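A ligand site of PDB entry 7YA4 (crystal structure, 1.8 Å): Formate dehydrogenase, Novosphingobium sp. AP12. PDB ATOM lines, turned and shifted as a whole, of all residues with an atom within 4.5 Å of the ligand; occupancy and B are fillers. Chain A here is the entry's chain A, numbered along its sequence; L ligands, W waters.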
ATOM      1  N   PHE A  99     -19.264 -21.317  26.765  1.00  0.00           N
ATOM      2  CA  PHE A  99     -19.560 -21.679  28.164  1.00  0.00           C
ATOM      3  C   PHE A  99     -18.282 -21.661  29.005  1.00  0.00           C
ATOM      4  O   PHE A  99     -18.343 -21.564  30.244  1.00  0.00           O
ATOM      5  CB  PHE A  99     -20.278 -23.037  28.238  1.00  0.00           C
ATOM      6  CG  PHE A  99     -21.184 -23.304  27.071  1.00  0.00           C
ATOM      7  CD1 PHE A  99     -22.309 -22.558  26.876  1.00  0.00           C
ATOM      8  CD2 PHE A  99     -20.760 -24.133  26.025  1.00  0.00           C
ATOM      9  CE1 PHE A  99     -23.071 -22.676  25.710  1.00  0.00           C
ATOM     10  CE2 PHE A  99     -21.521 -24.260  24.870  1.00  0.00           C
ATOM     11  CZ  PHE A  99     -22.671 -23.534  24.719  1.00  0.00           C
ATOM     12  N   ILE A 123     -22.762 -20.914  19.701  1.00  0.00           N
ATOM     13  CA  ILE A 123     -23.197 -19.715  19.020  1.00  0.00           C
ATOM     14  C   ILE A 123     -22.711 -18.514  19.820  1.00  0.00           C
ATOM     15  O   ILE A 123     -22.873 -18.502  21.040  1.00  0.00           O
ATOM     16  CB  ILE A 123     -24.720 -19.668  18.851  1.00  0.00           C
ATOM     17  CG1 ILE A 123     -25.283 -20.833  18.010  1.00  0.00           C
ATOM     18  CG2 ILE A 123     -25.146 -18.317  18.312  1.00  0.00           C
ATOM     19  CD1 ILE A 123     -26.810 -20.870  17.930  1.00  0.00           C
ATOM     20  N   GLY A 124     -22.130 -17.553  19.107  1.00  0.00           N
ATOM     21  CA  GLY A 124     -21.745 -16.260  19.637  1.00  0.00           C
ATOM     22  C   GLY A 124     -20.223 -16.211  19.757  1.00  0.00           C
ATOM     23  O   GLY A 124     -19.639 -16.930  20.587  1.00  0.00           O
ATOM     24  N   ASP A 126     -18.134 -13.473  20.225  1.00  0.00           N
ATOM     25  CA  ASP A 126     -17.685 -12.221  20.812  1.00  0.00           C
ATOM     26  C   ASP A 126     -16.452 -12.385  21.738  1.00  0.00           C
ATOM     27  O   ASP A 126     -15.840 -11.397  22.109  1.00  0.00           O
ATOM     28  CB  ASP A 126     -18.858 -11.630  21.612  1.00  0.00           C
ATOM     29  CG  ASP A 126     -19.528 -12.673  22.506  1.00  0.00           C
ATOM     30  OD1 ASP A 126     -19.066 -12.882  23.695  1.00  0.00           O
ATOM     31  OD2 ASP A 126     -20.482 -13.316  22.006  1.00  0.00           O
ATOM     32  N   ASN A 147     -28.093 -24.320  18.981  1.00  0.00           N
ATOM     33  CA  ASN A 147     -28.660 -24.419  20.319  1.00  0.00           C
ATOM     34  C   ASN A 147     -29.640 -23.267  20.590  1.00  0.00           C
ATOM     35  O   ASN A 147     -30.035 -23.041  21.746  1.00  0.00           O
ATOM     36  CB  ASN A 147     -27.554 -24.464  21.392  1.00  0.00           C
ATOM     37  CG  ASN A 147     -26.586 -23.310  21.304  1.00  0.00           C
ATOM     38  OD1 ASN A 147     -26.923 -22.313  20.693  1.00  0.00           O
ATOM     39  ND2 ASN A 147     -25.418 -23.398  21.947  1.00  0.00           N
ATOM     40  N   SER A 148     -30.081 -22.575  19.548  1.00  0.00           N
ATOM     41  CA  SER A 148     -31.002 -21.459  19.719  1.00  0.00           C
ATOM     42  C   SER A 148     -32.286 -21.904  20.443  1.00  0.00           C
ATOM     43  O   SER A 148     -32.837 -21.201  21.307  1.00  0.00           O
ATOM     44  CB  SER A 148     -31.328 -20.876  18.341  1.00  0.00           C
ATOM     45  OG  SER A 148     -30.161 -20.512  17.605  1.00  0.00           O
ATOM     46  N   VAL A 151     -31.797 -22.410  24.162  1.00  0.00           N
ATOM     47  CA  VAL A 151     -31.786 -21.169  24.923  1.00  0.00           C
ATOM     48  C   VAL A 151     -33.218 -20.650  25.126  1.00  0.00           C
ATOM     49  O   VAL A 151     -33.583 -20.170  26.196  1.00  0.00           O
ATOM     50  CB  VAL A 151     -30.887 -20.112  24.265  1.00  0.00           C
ATOM     51  CG1 VAL A 151     -30.832 -18.819  25.102  1.00  0.00           C
ATOM     52  CG2 VAL A 151     -29.496 -20.657  24.010  1.00  0.00           C
ATOM     53  N   ALA A 199     -34.171  -8.068  19.928  1.00  0.00           N
ATOM     54  CA  ALA A 199     -33.948  -8.918  18.767  1.00  0.00           C
ATOM     55  C   ALA A 199     -35.003 -10.013  18.638  1.00  0.00           C
ATOM     56  O   ALA A 199     -35.481 -10.596  19.609  1.00  0.00           O
ATOM     57  CB  ALA A 199     -32.569  -9.511  18.765  1.00  0.00           C
ATOM     58  N   ALA A 200     -35.272 -10.345  17.356  1.00  0.00           N
ATOM     59  CA  ALA A 200     -36.209 -11.372  16.971  1.00  0.00           C
ATOM     60  C   ALA A 200     -35.542 -12.293  15.933  1.00  0.00           C
ATOM     61  O   ALA A 200     -36.146 -12.665  14.924  1.00  0.00           O
ATOM     62  CB  ALA A 200     -37.487 -10.743  16.463  1.00  0.00           C
ATOM     63  N   GLY A 201     -34.296 -12.665  16.246  1.00  0.00           N
ATOM     64  CA  GLY A 201     -33.566 -13.712  15.551  1.00  0.00           C
ATOM     65  C   GLY A 201     -34.010 -15.088  16.006  1.00  0.00           C
ATOM     66  O   GLY A 201     -35.123 -15.272  16.464  1.00  0.00           O
ATOM     67  N   ARG A 202     -33.163 -16.097  15.819  1.00  0.00           N
ATOM     68  CA  ARG A 202     -33.623 -17.441  16.106  1.00  0.00           C
ATOM     69  C   ARG A 202     -34.125 -17.556  17.532  1.00  0.00           C
ATOM     70  O   ARG A 202     -35.164 -18.161  17.766  1.00  0.00           O
ATOM     71  CB  ARG A 202     -32.511 -18.449  15.843  1.00  0.00           C
ATOM     72  CG  ARG A 202     -32.173 -18.598  14.375  1.00  0.00           C
ATOM     73  CD  ARG A 202     -30.767 -19.217  14.203  1.00  0.00           C
ATOM     74  NE  ARG A 202     -30.391 -19.498  12.802  1.00  0.00           N
ATOM     75  CZ  ARG A 202     -29.918 -18.630  11.902  1.00  0.00           C
ATOM     76  NH1 ARG A 202     -29.511 -17.402  12.228  1.00  0.00           N
ATOM     77  NH2 ARG A 202     -29.757 -19.049  10.657  1.00  0.00           N
ATOM     78  N   ILE A 203     -33.363 -17.065  18.504  1.00  0.00           N
ATOM     79  CA  ILE A 203     -33.784 -17.267  19.886  1.00  0.00           C
ATOM     80  C   ILE A 203     -35.003 -16.393  20.240  1.00  0.00           C
ATOM     81  O   ILE A 203     -35.992 -16.897  20.812  1.00  0.00           O
ATOM     82  CB  ILE A 203     -32.605 -17.039  20.854  1.00  0.00           C
ATOM     83  CG1 ILE A 203     -31.472 -18.047  20.597  1.00  0.00           C
ATOM     84  CG2 ILE A 203     -33.109 -17.119  22.302  1.00  0.00           C
ATOM     85  CD1 ILE A 203     -30.219 -17.777  21.390  1.00  0.00           C
ATOM     86  N   TYR A 221     -38.189  -5.293  19.763  1.00  0.00           N
ATOM     87  CA  TYR A 221     -37.290  -4.345  19.142  1.00  0.00           C
ATOM     88  C   TYR A 221     -36.320  -5.073  18.201  1.00  0.00           C
ATOM     89  O   TYR A 221     -35.716  -6.085  18.551  1.00  0.00           O
ATOM     90  CB  TYR A 221     -36.539  -3.548  20.205  1.00  0.00           C
ATOM     91  CG  TYR A 221     -35.324  -2.854  19.637  1.00  0.00           C
ATOM     92  CD1 TYR A 221     -34.046  -3.369  19.808  1.00  0.00           C
ATOM     93  CD2 TYR A 221     -35.457  -1.703  18.878  1.00  0.00           C
ATOM     94  CE1 TYR A 221     -32.933  -2.769  19.242  1.00  0.00           C
ATOM     95  CE2 TYR A 221     -34.351  -1.085  18.300  1.00  0.00           C
ATOM     96  CZ  TYR A 221     -33.091  -1.606  18.508  1.00  0.00           C
ATOM     97  OH  TYR A 221     -32.002  -0.959  17.978  1.00  0.00           O
ATOM     98  N   ALA A 222     -36.139  -4.513  17.007  1.00  0.00           N
ATOM     99  CA  ALA A 222     -35.106  -5.013  16.121  1.00  0.00           C
ATOM    100  C   ALA A 222     -34.724  -3.908  15.144  1.00  0.00           C
ATOM    101  O   ALA A 222     -35.439  -2.892  15.055  1.00  0.00           O
ATOM    102  CB  ALA A 222     -35.608  -6.226  15.399  1.00  0.00           C
ATOM    103  N   ARG A 223     -33.645  -4.126  14.394  1.00  0.00           N
ATOM    104  CA  ARG A 223     -33.164  -3.136  13.449  1.00  0.00           C
ATOM    105  C   ARG A 223     -33.988  -3.251  12.164  1.00  0.00           C
ATOM    106  O   ARG A 223     -34.111  -2.284  11.422  1.00  0.00           O
ATOM    107  CB  ARG A 223     -31.652  -3.276  13.167  1.00  0.00           C
ATOM    108  CG  ARG A 223     -30.757  -3.087  14.390  1.00  0.00           C
ATOM    109  CD  ARG A 223     -29.318  -3.429  14.123  1.00  0.00           C
ATOM    110  NE  ARG A 223     -29.142  -4.833  13.747  1.00  0.00           N
ATOM    111  CZ  ARG A 223     -28.025  -5.345  13.245  1.00  0.00           C
ATOM    112  NH1 ARG A 223     -26.906  -4.631  13.273  1.00  0.00           N
ATOM    113  NH2 ARG A 223     -28.044  -6.596  12.782  1.00  0.00           N
ATOM    114  N   ASN A 255     -31.910 -10.947  23.488  1.00  0.00           N
ATOM    115  CA  ASN A 255     -31.643 -12.055  22.567  1.00  0.00           C
ATOM    116  C   ASN A 255     -30.829 -11.634  21.326  1.00  0.00           C
ATOM    117  O   ASN A 255     -30.927 -12.285  20.274  1.00  0.00           O
ATOM    118  CB  ASN A 255     -32.947 -12.728  22.171  1.00  0.00           C
ATOM    119  CG  ASN A 255     -33.722 -13.281  23.355  1.00  0.00           C
ATOM    120  OD1 ASN A 255     -34.771 -12.733  23.752  1.00  0.00           O
ATOM    121  ND2 ASN A 255     -33.177 -14.298  23.968  1.00  0.00           N
ATOM    122  N   ALA A 256     -29.977 -10.623  21.502  1.00  0.00           N
ATOM    123  CA  ALA A 256     -29.119 -10.060  20.464  1.00  0.00           C
ATOM    124  C   ALA A 256     -27.696 -10.544  20.684  1.00  0.00           C
ATOM    125  O   ALA A 256     -27.300 -10.801  21.823  1.00  0.00           O
ATOM    126  CB  ALA A 256     -29.173  -8.549  20.494  1.00  0.00           C
ATOM    127  N   PRO A 257     -26.837 -10.576  19.626  1.00  0.00           N
ATOM    128  CA  PRO A 257     -25.397 -10.820  19.797  1.00  0.00           C
ATOM    129  C   PRO A 257     -24.697  -9.648  20.466  1.00  0.00           C
ATOM    130  O   PRO A 257     -25.237  -8.549  20.468  1.00  0.00           O
ATOM    131  CB  PRO A 257     -24.875 -10.986  18.366  1.00  0.00           C
ATOM    132  CG  PRO A 257     -26.118 -11.079  17.500  1.00  0.00           C
ATOM    133  CD  PRO A 257     -27.165 -10.265  18.227  1.00  0.00           C
ATOM    134  N   HIS A 259     -21.870  -6.975  20.288  1.00  0.00           N
ATOM    135  CA  HIS A 259     -21.017  -6.208  19.421  1.00  0.00           C
ATOM    136  C   HIS A 259     -21.242  -4.731  19.756  1.00  0.00           C
ATOM    137  O   HIS A 259     -22.001  -4.439  20.675  1.00  0.00           O
ATOM    138  CB  HIS A 259     -21.323  -6.575  17.963  1.00  0.00           C
ATOM    139  CG  HIS A 259     -22.699  -6.226  17.492  1.00  0.00           C
ATOM    140  ND1 HIS A 259     -22.985  -5.049  16.859  1.00  0.00           N
ATOM    141  CD2 HIS A 259     -23.849  -6.973  17.516  1.00  0.00           C
ATOM    142  CE1 HIS A 259     -24.265  -5.056  16.503  1.00  0.00           C
ATOM    143  NE2 HIS A 259     -24.840  -6.231  16.931  1.00  0.00           N
ATOM    144  N   GLU A 261     -22.932  -2.166  18.889  1.00  0.00           N
ATOM    145  CA  GLU A 261     -24.291  -1.653  19.008  1.00  0.00           C
ATOM    146  C   GLU A 261     -25.017  -2.119  20.270  1.00  0.00           C
ATOM    147  O   GLU A 261     -25.880  -1.421  20.803  1.00  0.00           O
ATOM    148  CB  GLU A 261     -25.137  -2.116  17.829  1.00  0.00           C
ATOM    149  CG  GLU A 261     -24.741  -1.470  16.538  1.00  0.00           C
ATOM    150  CD  GLU A 261     -25.654  -1.808  15.367  1.00  0.00           C
ATOM    151  OE1 GLU A 261     -26.382  -2.812  15.441  1.00  0.00           O
ATOM    152  OE2 GLU A 261     -25.608  -1.095  14.370  1.00  0.00           O
ATOM    153  N   THR A 262     -24.688  -3.321  20.757  1.00  0.00           N
ATOM    154  CA  THR A 262     -25.420  -3.881  21.880  1.00  0.00           C
ATOM    155  C   THR A 262     -24.638  -3.785  23.184  1.00  0.00           C
ATOM    156  O   THR A 262     -25.193  -4.050  24.250  1.00  0.00           O
ATOM    157  CB  THR A 262     -25.863  -5.314  21.610  1.00  0.00           C
ATOM    158  OG1 THR A 262     -24.682  -6.122  21.434  1.00  0.00           O
ATOM    159  CG2 THR A 262     -26.799  -5.419  20.420  1.00  0.00           C
ATOM    160  N   MET A 265     -26.074  -1.774  26.180  1.00  0.00           N
ATOM    161  CA  MET A 265     -27.349  -1.212  25.784  1.00  0.00           C
ATOM    162  C   MET A 265     -28.213  -1.030  27.033  1.00  0.00           C
ATOM    163  O   MET A 265     -28.887   0.014  27.163  1.00  0.00           O
ATOM    164  CB  MET A 265     -28.062  -2.118  24.789  1.00  0.00           C
ATOM    165  CG  MET A 265     -29.515  -1.770  24.598  1.00  0.00           C
ATOM    166  SD  MET A 265     -30.264  -2.855  23.318  1.00  0.00           S
ATOM    167  CE  MET A 265     -29.509  -2.344  21.786  1.00  0.00           C
ATOM    168  N   THR A 283     -30.220 -14.326  28.442  1.00  0.00           N
ATOM    169  CA  THR A 283     -29.547 -15.532  28.038  1.00  0.00           C
ATOM    170  C   THR A 283     -28.700 -15.275  26.779  1.00  0.00           C
ATOM    171  O   THR A 283     -28.281 -16.225  26.141  1.00  0.00           O
ATOM    172  CB  THR A 283     -30.584 -16.606  27.686  1.00  0.00           C
ATOM    173  OG1 THR A 283     -31.514 -16.163  26.694  1.00  0.00           O
ATOM    174  CG2 THR A 283     -31.354 -17.040  28.918  1.00  0.00           C
ATOM    175  N   ALA A 284     -28.485 -13.990  26.436  1.00  0.00           N
ATOM    176  CA  ALA A 284     -27.720 -13.634  25.242  1.00  0.00           C
ATOM    177  C   ALA A 284     -26.237 -13.491  25.615  1.00  0.00           C
ATOM    178  O   ALA A 284     -25.480 -14.478  25.539  1.00  0.00           O
ATOM    179  CB  ALA A 284     -28.332 -12.385  24.600  1.00  0.00           C
ATOM    180  N   ARG A 285     -25.820 -12.311  26.076  1.00  0.00           N
ATOM    181  CA  ARG A 285     -24.459 -12.102  26.595  1.00  0.00           C
ATOM    182  C   ARG A 285     -24.593 -11.131  27.753  1.00  0.00           C
ATOM    183  O   ARG A 285     -25.345 -10.143  27.684  1.00  0.00           O
ATOM    184  CB  ARG A 285     -23.506 -11.573  25.528  1.00  0.00           C
ATOM    185  CG  ARG A 285     -23.100 -12.590  24.481  1.00  0.00           C
ATOM    186  CD  ARG A 285     -22.337 -13.747  25.074  1.00  0.00           C
ATOM    187  NE  ARG A 285     -21.854 -14.679  24.050  1.00  0.00           N
ATOM    188  CZ  ARG A 285     -22.309 -15.912  23.825  1.00  0.00           C
ATOM    189  NH1 ARG A 285     -23.418 -16.373  24.408  1.00  0.00           N
ATOM    190  NH2 ARG A 285     -21.650 -16.663  22.956  1.00  0.00           N
ATOM    191  N   ASP A 309     -28.132 -16.992  32.099  1.00  0.00           N
ATOM    192  CA  ASP A 309     -27.077 -18.000  32.246  1.00  0.00           C
ATOM    193  C   ASP A 309     -25.705 -17.448  31.838  1.00  0.00           C
ATOM    194  O   ASP A 309     -24.690 -18.140  31.996  1.00  0.00           O
ATOM    195  CB  ASP A 309     -27.386 -19.290  31.478  1.00  0.00           C
ATOM    196  CG  ASP A 309     -27.581 -19.122  29.995  1.00  0.00           C
ATOM    197  OD1 ASP A 309     -27.959 -17.994  29.575  1.00  0.00           O
ATOM    198  OD2 ASP A 309     -27.344 -20.148  29.276  1.00  0.00           O
ATOM    199  N   VAL A 310     -25.670 -16.188  31.355  1.00  0.00           N
ATOM    200  CA  VAL A 310     -24.444 -15.619  30.816  1.00  0.00           C
ATOM    201  C   VAL A 310     -23.877 -14.534  31.748  1.00  0.00           C
ATOM    202  O   VAL A 310     -24.607 -13.711  32.321  1.00  0.00           O
ATOM    203  CB  VAL A 310     -24.657 -15.132  29.382  1.00  0.00           C
ATOM    204  CG1 VAL A 310     -24.987 -16.258  28.428  1.00  0.00           C
ATOM    205  CG2 VAL A 310     -25.786 -14.073  29.321  1.00  0.00           C
ATOM    206  N   HIS A 333     -23.251 -20.752  32.724  1.00  0.00           N
ATOM    207  CA  HIS A 333     -23.587 -20.705  31.303  1.00  0.00           C
ATOM    208  C   HIS A 333     -23.829 -22.108  30.756  1.00  0.00           C
ATOM    209  O   HIS A 333     -22.904 -22.799  30.321  1.00  0.00           O
ATOM    210  CB  HIS A 333     -22.507 -19.925  30.559  1.00  0.00           C
ATOM    211  CG  HIS A 333     -22.825 -19.635  29.121  1.00  0.00           C
ATOM    212  ND1 HIS A 333     -21.954 -19.051  28.242  1.00  0.00           N
ATOM    213  CD2 HIS A 333     -23.952 -19.947  28.412  1.00  0.00           C
ATOM    214  CE1 HIS A 333     -22.541 -18.960  27.057  1.00  0.00           C
ATOM    215  NE2 HIS A 333     -23.750 -19.531  27.124  1.00  0.00           N
ATOM    216  N   SER A 335     -27.299 -23.083  29.027  1.00  0.00           N
ATOM    217  CA  SER A 335     -28.487 -23.347  28.200  1.00  0.00           C
ATOM    218  C   SER A 335     -28.077 -23.898  26.850  1.00  0.00           C
ATOM    219  O   SER A 335     -28.634 -24.910  26.410  1.00  0.00           O
ATOM    220  CB  SER A 335     -29.431 -22.159  28.069  1.00  0.00           C
ATOM    221  OG  SER A 335     -28.852 -21.099  27.348  1.00  0.00           O
ATOM    222  N   GLY A 336     -27.021 -23.342  26.236  1.00  0.00           N
ATOM    223  CA  GLY A 336     -26.611 -23.755  24.922  1.00  0.00           C
ATOM    224  C   GLY A 336     -25.832 -25.081  24.944  1.00  0.00           C
ATOM    225  O   GLY A 336     -25.512 -25.593  23.882  1.00  0.00           O
ATOM    226  N   THR A 377     -23.279 -14.749   8.275  1.00  0.00           N
ATOM    227  CA  THR A 377     -24.044 -14.368   9.464  1.00  0.00           C
ATOM    228  C   THR A 377     -23.387 -13.180  10.175  1.00  0.00           C
ATOM    229  O   THR A 377     -24.102 -12.306  10.722  1.00  0.00           O
ATOM    230  CB  THR A 377     -24.284 -15.564  10.393  1.00  0.00           C
ATOM    231  OG1 THR A 377     -25.143 -16.520   9.762  1.00  0.00           O
ATOM    232  CG2 THR A 377     -24.874 -15.181  11.742  1.00  0.00           C
ATOM    233  N   LEU A 380     -24.599  -9.996   8.731  1.00  0.00           N
ATOM    234  CA  LEU A 380     -26.007  -9.761   9.002  1.00  0.00           C
ATOM    235  C   LEU A 380     -26.240  -9.305  10.436  1.00  0.00           C
ATOM    236  O   LEU A 380     -27.166  -8.544  10.666  1.00  0.00           O
ATOM    237  CB  LEU A 380     -26.826 -11.029   8.773  1.00  0.00           C
ATOM    238  CG  LEU A 380     -26.909 -11.574   7.346  1.00  0.00           C
ATOM    239  CD1 LEU A 380     -27.604 -12.925   7.364  1.00  0.00           C
ATOM    240  CD2 LEU A 380     -27.654 -10.630   6.420  1.00  0.00           C
ATOM    241  N   SER A 381     -25.460  -9.838  11.386  1.00  0.00           N
ATOM    242  CA  SER A 381     -25.865  -9.794  12.792  1.00  0.00           C
ATOM    243  C   SER A 381     -24.819  -9.146  13.699  1.00  0.00           C
ATOM    244  O   SER A 381     -25.137  -8.869  14.857  1.00  0.00           O
ATOM    245  CB  SER A 381     -26.217 -11.175  13.302  1.00  0.00           C
ATOM    246  OG  SER A 381     -27.461 -11.600  12.724  1.00  0.00           O
ATOM    247  N   TYR A 382     -23.620  -8.878  13.195  1.00  0.00           N
ATOM    248  CA  TYR A 382     -22.598  -8.198  13.962  1.00  0.00           C
ATOM    249  C   TYR A 382     -22.188  -6.896  13.268  1.00  0.00           C
ATOM    250  O   TYR A 382     -22.493  -6.677  12.079  1.00  0.00           O
ATOM    251  CB  TYR A 382     -21.350  -9.076  14.133  1.00  0.00           C
ATOM    252  CG  TYR A 382     -21.496 -10.271  15.055  1.00  0.00           C
ATOM    253  CD1 TYR A 382     -22.278 -11.374  14.718  1.00  0.00           C
ATOM    254  CD2 TYR A 382     -20.897 -10.270  16.318  1.00  0.00           C
ATOM    255  CE1 TYR A 382     -22.422 -12.464  15.562  1.00  0.00           C
ATOM    256  CE2 TYR A 382     -21.082 -11.322  17.194  1.00  0.00           C
ATOM    257  CZ  TYR A 382     -21.826 -12.432  16.815  1.00  0.00           C
ATOM    258  OH  TYR A 382     -21.967 -13.435  17.735  1.00  0.00           O
HETATM  259  P1  LIG L   1     -29.403 -14.945  15.271  1.00  0.00           P
HETATM  260  O1  LIG L   1     -28.250 -14.449  14.463  1.00  0.00           O
HETATM  261  O2  LIG L   1     -30.368 -15.856  14.604  1.00  0.00           O
HETATM  262  O3  LIG L   1     -30.225 -13.730  15.855  1.00  0.00           O
HETATM  263  C1  LIG L   1     -29.597 -12.566  16.340  1.00  0.00           C
HETATM  264  C2  LIG L   1     -30.491 -11.419  15.982  1.00  0.00           C
HETATM  265  O4  LIG L   1     -29.974 -10.258  16.665  1.00  0.00           O
HETATM  266  C3  LIG L   1     -30.567 -11.048  14.486  1.00  0.00           C
HETATM  267  O5  LIG L   1     -31.912 -10.909  14.005  1.00  0.00           O
HETATM  268  C4  LIG L   1     -29.827  -9.713  14.417  1.00  0.00           C
HETATM  269  O6  LIG L   1     -30.284  -8.848  13.398  1.00  0.00           O
HETATM  270  C5  LIG L   1     -30.173  -9.172  15.804  1.00  0.00           C
HETATM  271  N1  LIG L   1     -29.384  -8.026  16.207  1.00  0.00           N
HETATM  272  C6  LIG L   1     -28.067  -7.757  15.940  1.00  0.00           C
HETATM  273  N2  LIG L   1     -27.697  -6.590  16.389  1.00  0.00           N
HETATM  274  C7  LIG L   1     -28.827  -6.054  16.971  1.00  0.00           C
HETATM  275  C8  LIG L   1     -29.078  -4.829  17.621  1.00  0.00           C
HETATM  276  N3  LIG L   1     -28.175  -3.866  17.747  1.00  0.00           N
HETATM  277  N4  LIG L   1     -30.303  -4.646  18.166  1.00  0.00           N
HETATM  278  C9  LIG L   1     -31.227  -5.594  17.963  1.00  0.00           C
HETATM  279  N5  LIG L   1     -31.124  -6.777  17.348  1.00  0.00           N
HETATM  280  C10 LIG L   1     -29.871  -6.939  16.873  1.00  0.00           C
HETATM  281  O7  LIG L   1     -28.774 -15.556  16.655  1.00  0.00           O
HETATM  282  P2  LIG L   1     -29.459 -16.413  17.831  1.00  0.00           P
HETATM  283  O8  LIG L   1     -29.267 -17.875  17.591  1.00  0.00           O
HETATM  284  O9  LIG L   1     -30.856 -15.866  18.023  1.00  0.00           O
HETATM  285  O10 LIG L   1     -28.507 -15.972  19.048  1.00  0.00           O
HETATM  286  C11 LIG L   1     -28.479 -14.623  19.548  1.00  0.00           C
HETATM  287  C12 LIG L   1     -27.359 -14.500  20.548  1.00  0.00           C
HETATM  288  O11 LIG L   1     -27.706 -15.268  21.723  1.00  0.00           O
HETATM  289  C13 LIG L   1     -25.984 -15.025  20.103  1.00  0.00           C
HETATM  290  O12 LIG L   1     -25.282 -14.079  19.317  1.00  0.00           O
HETATM  291  C14 LIG L   1     -25.310 -15.339  21.437  1.00  0.00           C
HETATM  292  O13 LIG L   1     -24.603 -14.215  21.920  1.00  0.00           O
HETATM  293  C15 LIG L   1     -26.499 -15.686  22.344  1.00  0.00           C
HETATM  294  N6  LIG L   1     -26.571 -17.141  22.615  1.00  0.00           N
HETATM  295  C16 LIG L   1     -26.552 -17.582  23.907  1.00  0.00           C
HETATM  296  C17 LIG L   1     -26.567 -18.942  24.175  1.00  0.00           C
HETATM  297  C18 LIG L   1     -26.568 -19.414  25.595  1.00  0.00           C
HETATM  298  O14 LIG L   1     -26.991 -18.662  26.535  1.00  0.00           O
HETATM  299  N7  LIG L   1     -26.120 -20.628  25.804  1.00  0.00           N
HETATM  300  C19 LIG L   1     -26.586 -19.857  23.124  1.00  0.00           C
HETATM  301  C20 LIG L   1     -26.627 -19.394  21.826  1.00  0.00           C
HETATM  302  C21 LIG L   1     -26.649 -18.039  21.580  1.00  0.00           C
HETATM  303  O   HOH W   1     -23.979 -15.110  16.963  1.00  0.00           O
HETATM  304  O   HOH W   2     -32.431 -12.317  12.009  1.00  0.00           O
HETATM  305  O   HOH W   3     -22.573 -12.656  20.521  1.00  0.00           O
HETATM  306  O   HOH W   4     -32.005 -15.189  12.690  1.00  0.00           O
HETATM  307  O   HOH W   5     -29.229  -1.113  18.036  1.00  0.00           O
HETATM  308  O   HOH W   6     -27.572 -18.610  15.485  1.00  0.00           O
HETATM  309  O   HOH W   7     -33.941  -9.265  15.033  1.00  0.00           O
HETATM  310  O   HOH W   8     -32.146  -6.466  14.485  1.00  0.00           O
HETATM  311  O   HOH W   9     -32.550 -13.665  18.559  1.00  0.00           O
HETATM  312  O   HOH W  10     -28.439 -13.815  11.841  1.00  0.00           O
HETATM  313  O   HOH W  11     -25.562 -14.618  14.933  1.00  0.00           O
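OG of Ser 148 is in hydrogen-bond range of O8 of the ligand, 2.8 Å away.
A ring nitrogen (NE2) of His 259 sits at hydrogen-bond distance from a nitrogen (N2) of the ligand (2.9 Å).
NE2 of His 333 lies within hydrogen-bond range of N7 of the ligand, at 2.9 Å.
The backbone NH (N) of Arg 202 is in hydrogen-bond range of an oxygen (O2) of the ligand, 3.1 Å away.
An oxygen (O6) of the ligand lies within hydrogen-bond range of the guanidinium group (NH2) of Arg 223, 3.2 Å away.
OG of Ser 335 sits at hydrogen-bond distance from O14 of the ligand, 3.2 Å away.
The backbone NH of Ile 203 is in hydrogen-bond range of an oxygen (O9) of the ligand, at 2.8 Å.
The guanidinium group of Arg 202 is in salt-bridge range of an oxygen (O2) of the ligand.
OG of Ser 381 is in hydrogen-bond range of O1 of the ligand (3.4 Å).
The side-chain carboxylate (OE1) of Glu 261 is in hydrogen-bond range of a nitrogen (N3) of the ligand (3.1 Å).
A ring nitrogen (NE2) of His 259 sits at hydrogen-bond distance from the backbone carbonyl oxygen (O) of Ser 381 (3.4 Å).
N of Ala 199 lies within hydrogen-bond range of O of Tyr 221 (2.9 Å).
OE1 of Glu 261 lies within salt-bridge range of NH1 of Arg 223.
The backbone carbonyl oxygen of Asp 309 sits close to the backbone NH of His 333 (3.1 Å).
The guanidinium group (NH2) of Arg 223 is in hydrogen-bond range of the backbone carbonyl oxygen (O) of Leu 380 (3.0 Å).
The guanidinium group of Arg 285 lies within hydrogen-bond range of the backbone carbonyl oxygen of Ile 123 (2.9 Å).
The guanidinium group of Arg 285 lies within salt-bridge range of the side-chain carboxylate of Asp 126 (2.8 Å).
The backbone carbonyl oxygen (O) of Pro 257 lies within hydrogen-bond range of the side-chain hydroxyl (OG1) of Thr 262 (2.7 Å).
An oxygen (O14) of the ligand lies close to the backbone carbonyl oxygen of Thr 283 (2.8 Å).
An oxygen (O14) of the ligand lies close to the side-chain carboxylate of Asp 309.
A nitrogen (N7) of the ligand lies close to the backbone NH (N) of Gly 336.
Merely in contact with the ligand: Asn 147 (3.1 Å), Val 151 (3.1 Å), Pro 257 (3.2 Å), Gly 201 (3.4 Å), Thr 262 (3.4 Å), Arg 285 (3.4 Å), Ala 199 (3.4 Å), Tyr 221 (3.4 Å), Asn 255 (3.5 Å), Ile 123 (3.5 Å), Ala 284 (3.6 Å), Val 310 (3.7 Å), Phe 99 (3.7 Å), Tyr 382 (3.7 Å) and Ala 256 (3.9 Å).
Within 4 Å of the ligand: Phe 99, Ile 123, Asn 147, Ser 148, Val 151, Ala 199, Gly 201, Arg 202, Ile 203, Tyr 221, Arg 223, Asn 255, Ala 256, Pro 257, His 259, Glu 261, Thr 262, Thr 283, Ala 284, Arg 285, Asp 309, Val 310, His 333, Ser 335, Gly 336, Ser 381 and Tyr 382.
Water W4 bridges an oxygen (O2) of the ligand and the guanidinium group of Arg 202.
Water W10 lies within hydrogen-bond range of the side-chain hydroxyl (OG) of Ser 381 (2.6 Å) and an oxygen (O1) of the ligand (2.7 Å).
Water W9 lies within hydrogen-bond range of the backbone carbonyl oxygen of Asn 255 (2.7 Å), an oxygen (O9) of the ligand (2.8 Å), the backbone NH of Gly 201 (3.1 Å) and the backbone NH of Ile 203 (3.5 Å).
Water W1 bridges the side-chain hydroxyl (OH) of Tyr 382 (2.7 Å) and an oxygen (O12) of the ligand (2.9 Å).
Water W3 lies within hydrogen-bond range of the side-chain carboxylate of Asp 126, an oxygen (O13) of the ligand and the side-chain hydroxyl of Tyr 382.
Water W8 lies within hydrogen-bond range of N of Arg 223 (2.8 Å) and N5 of the ligand (3.1 Å).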
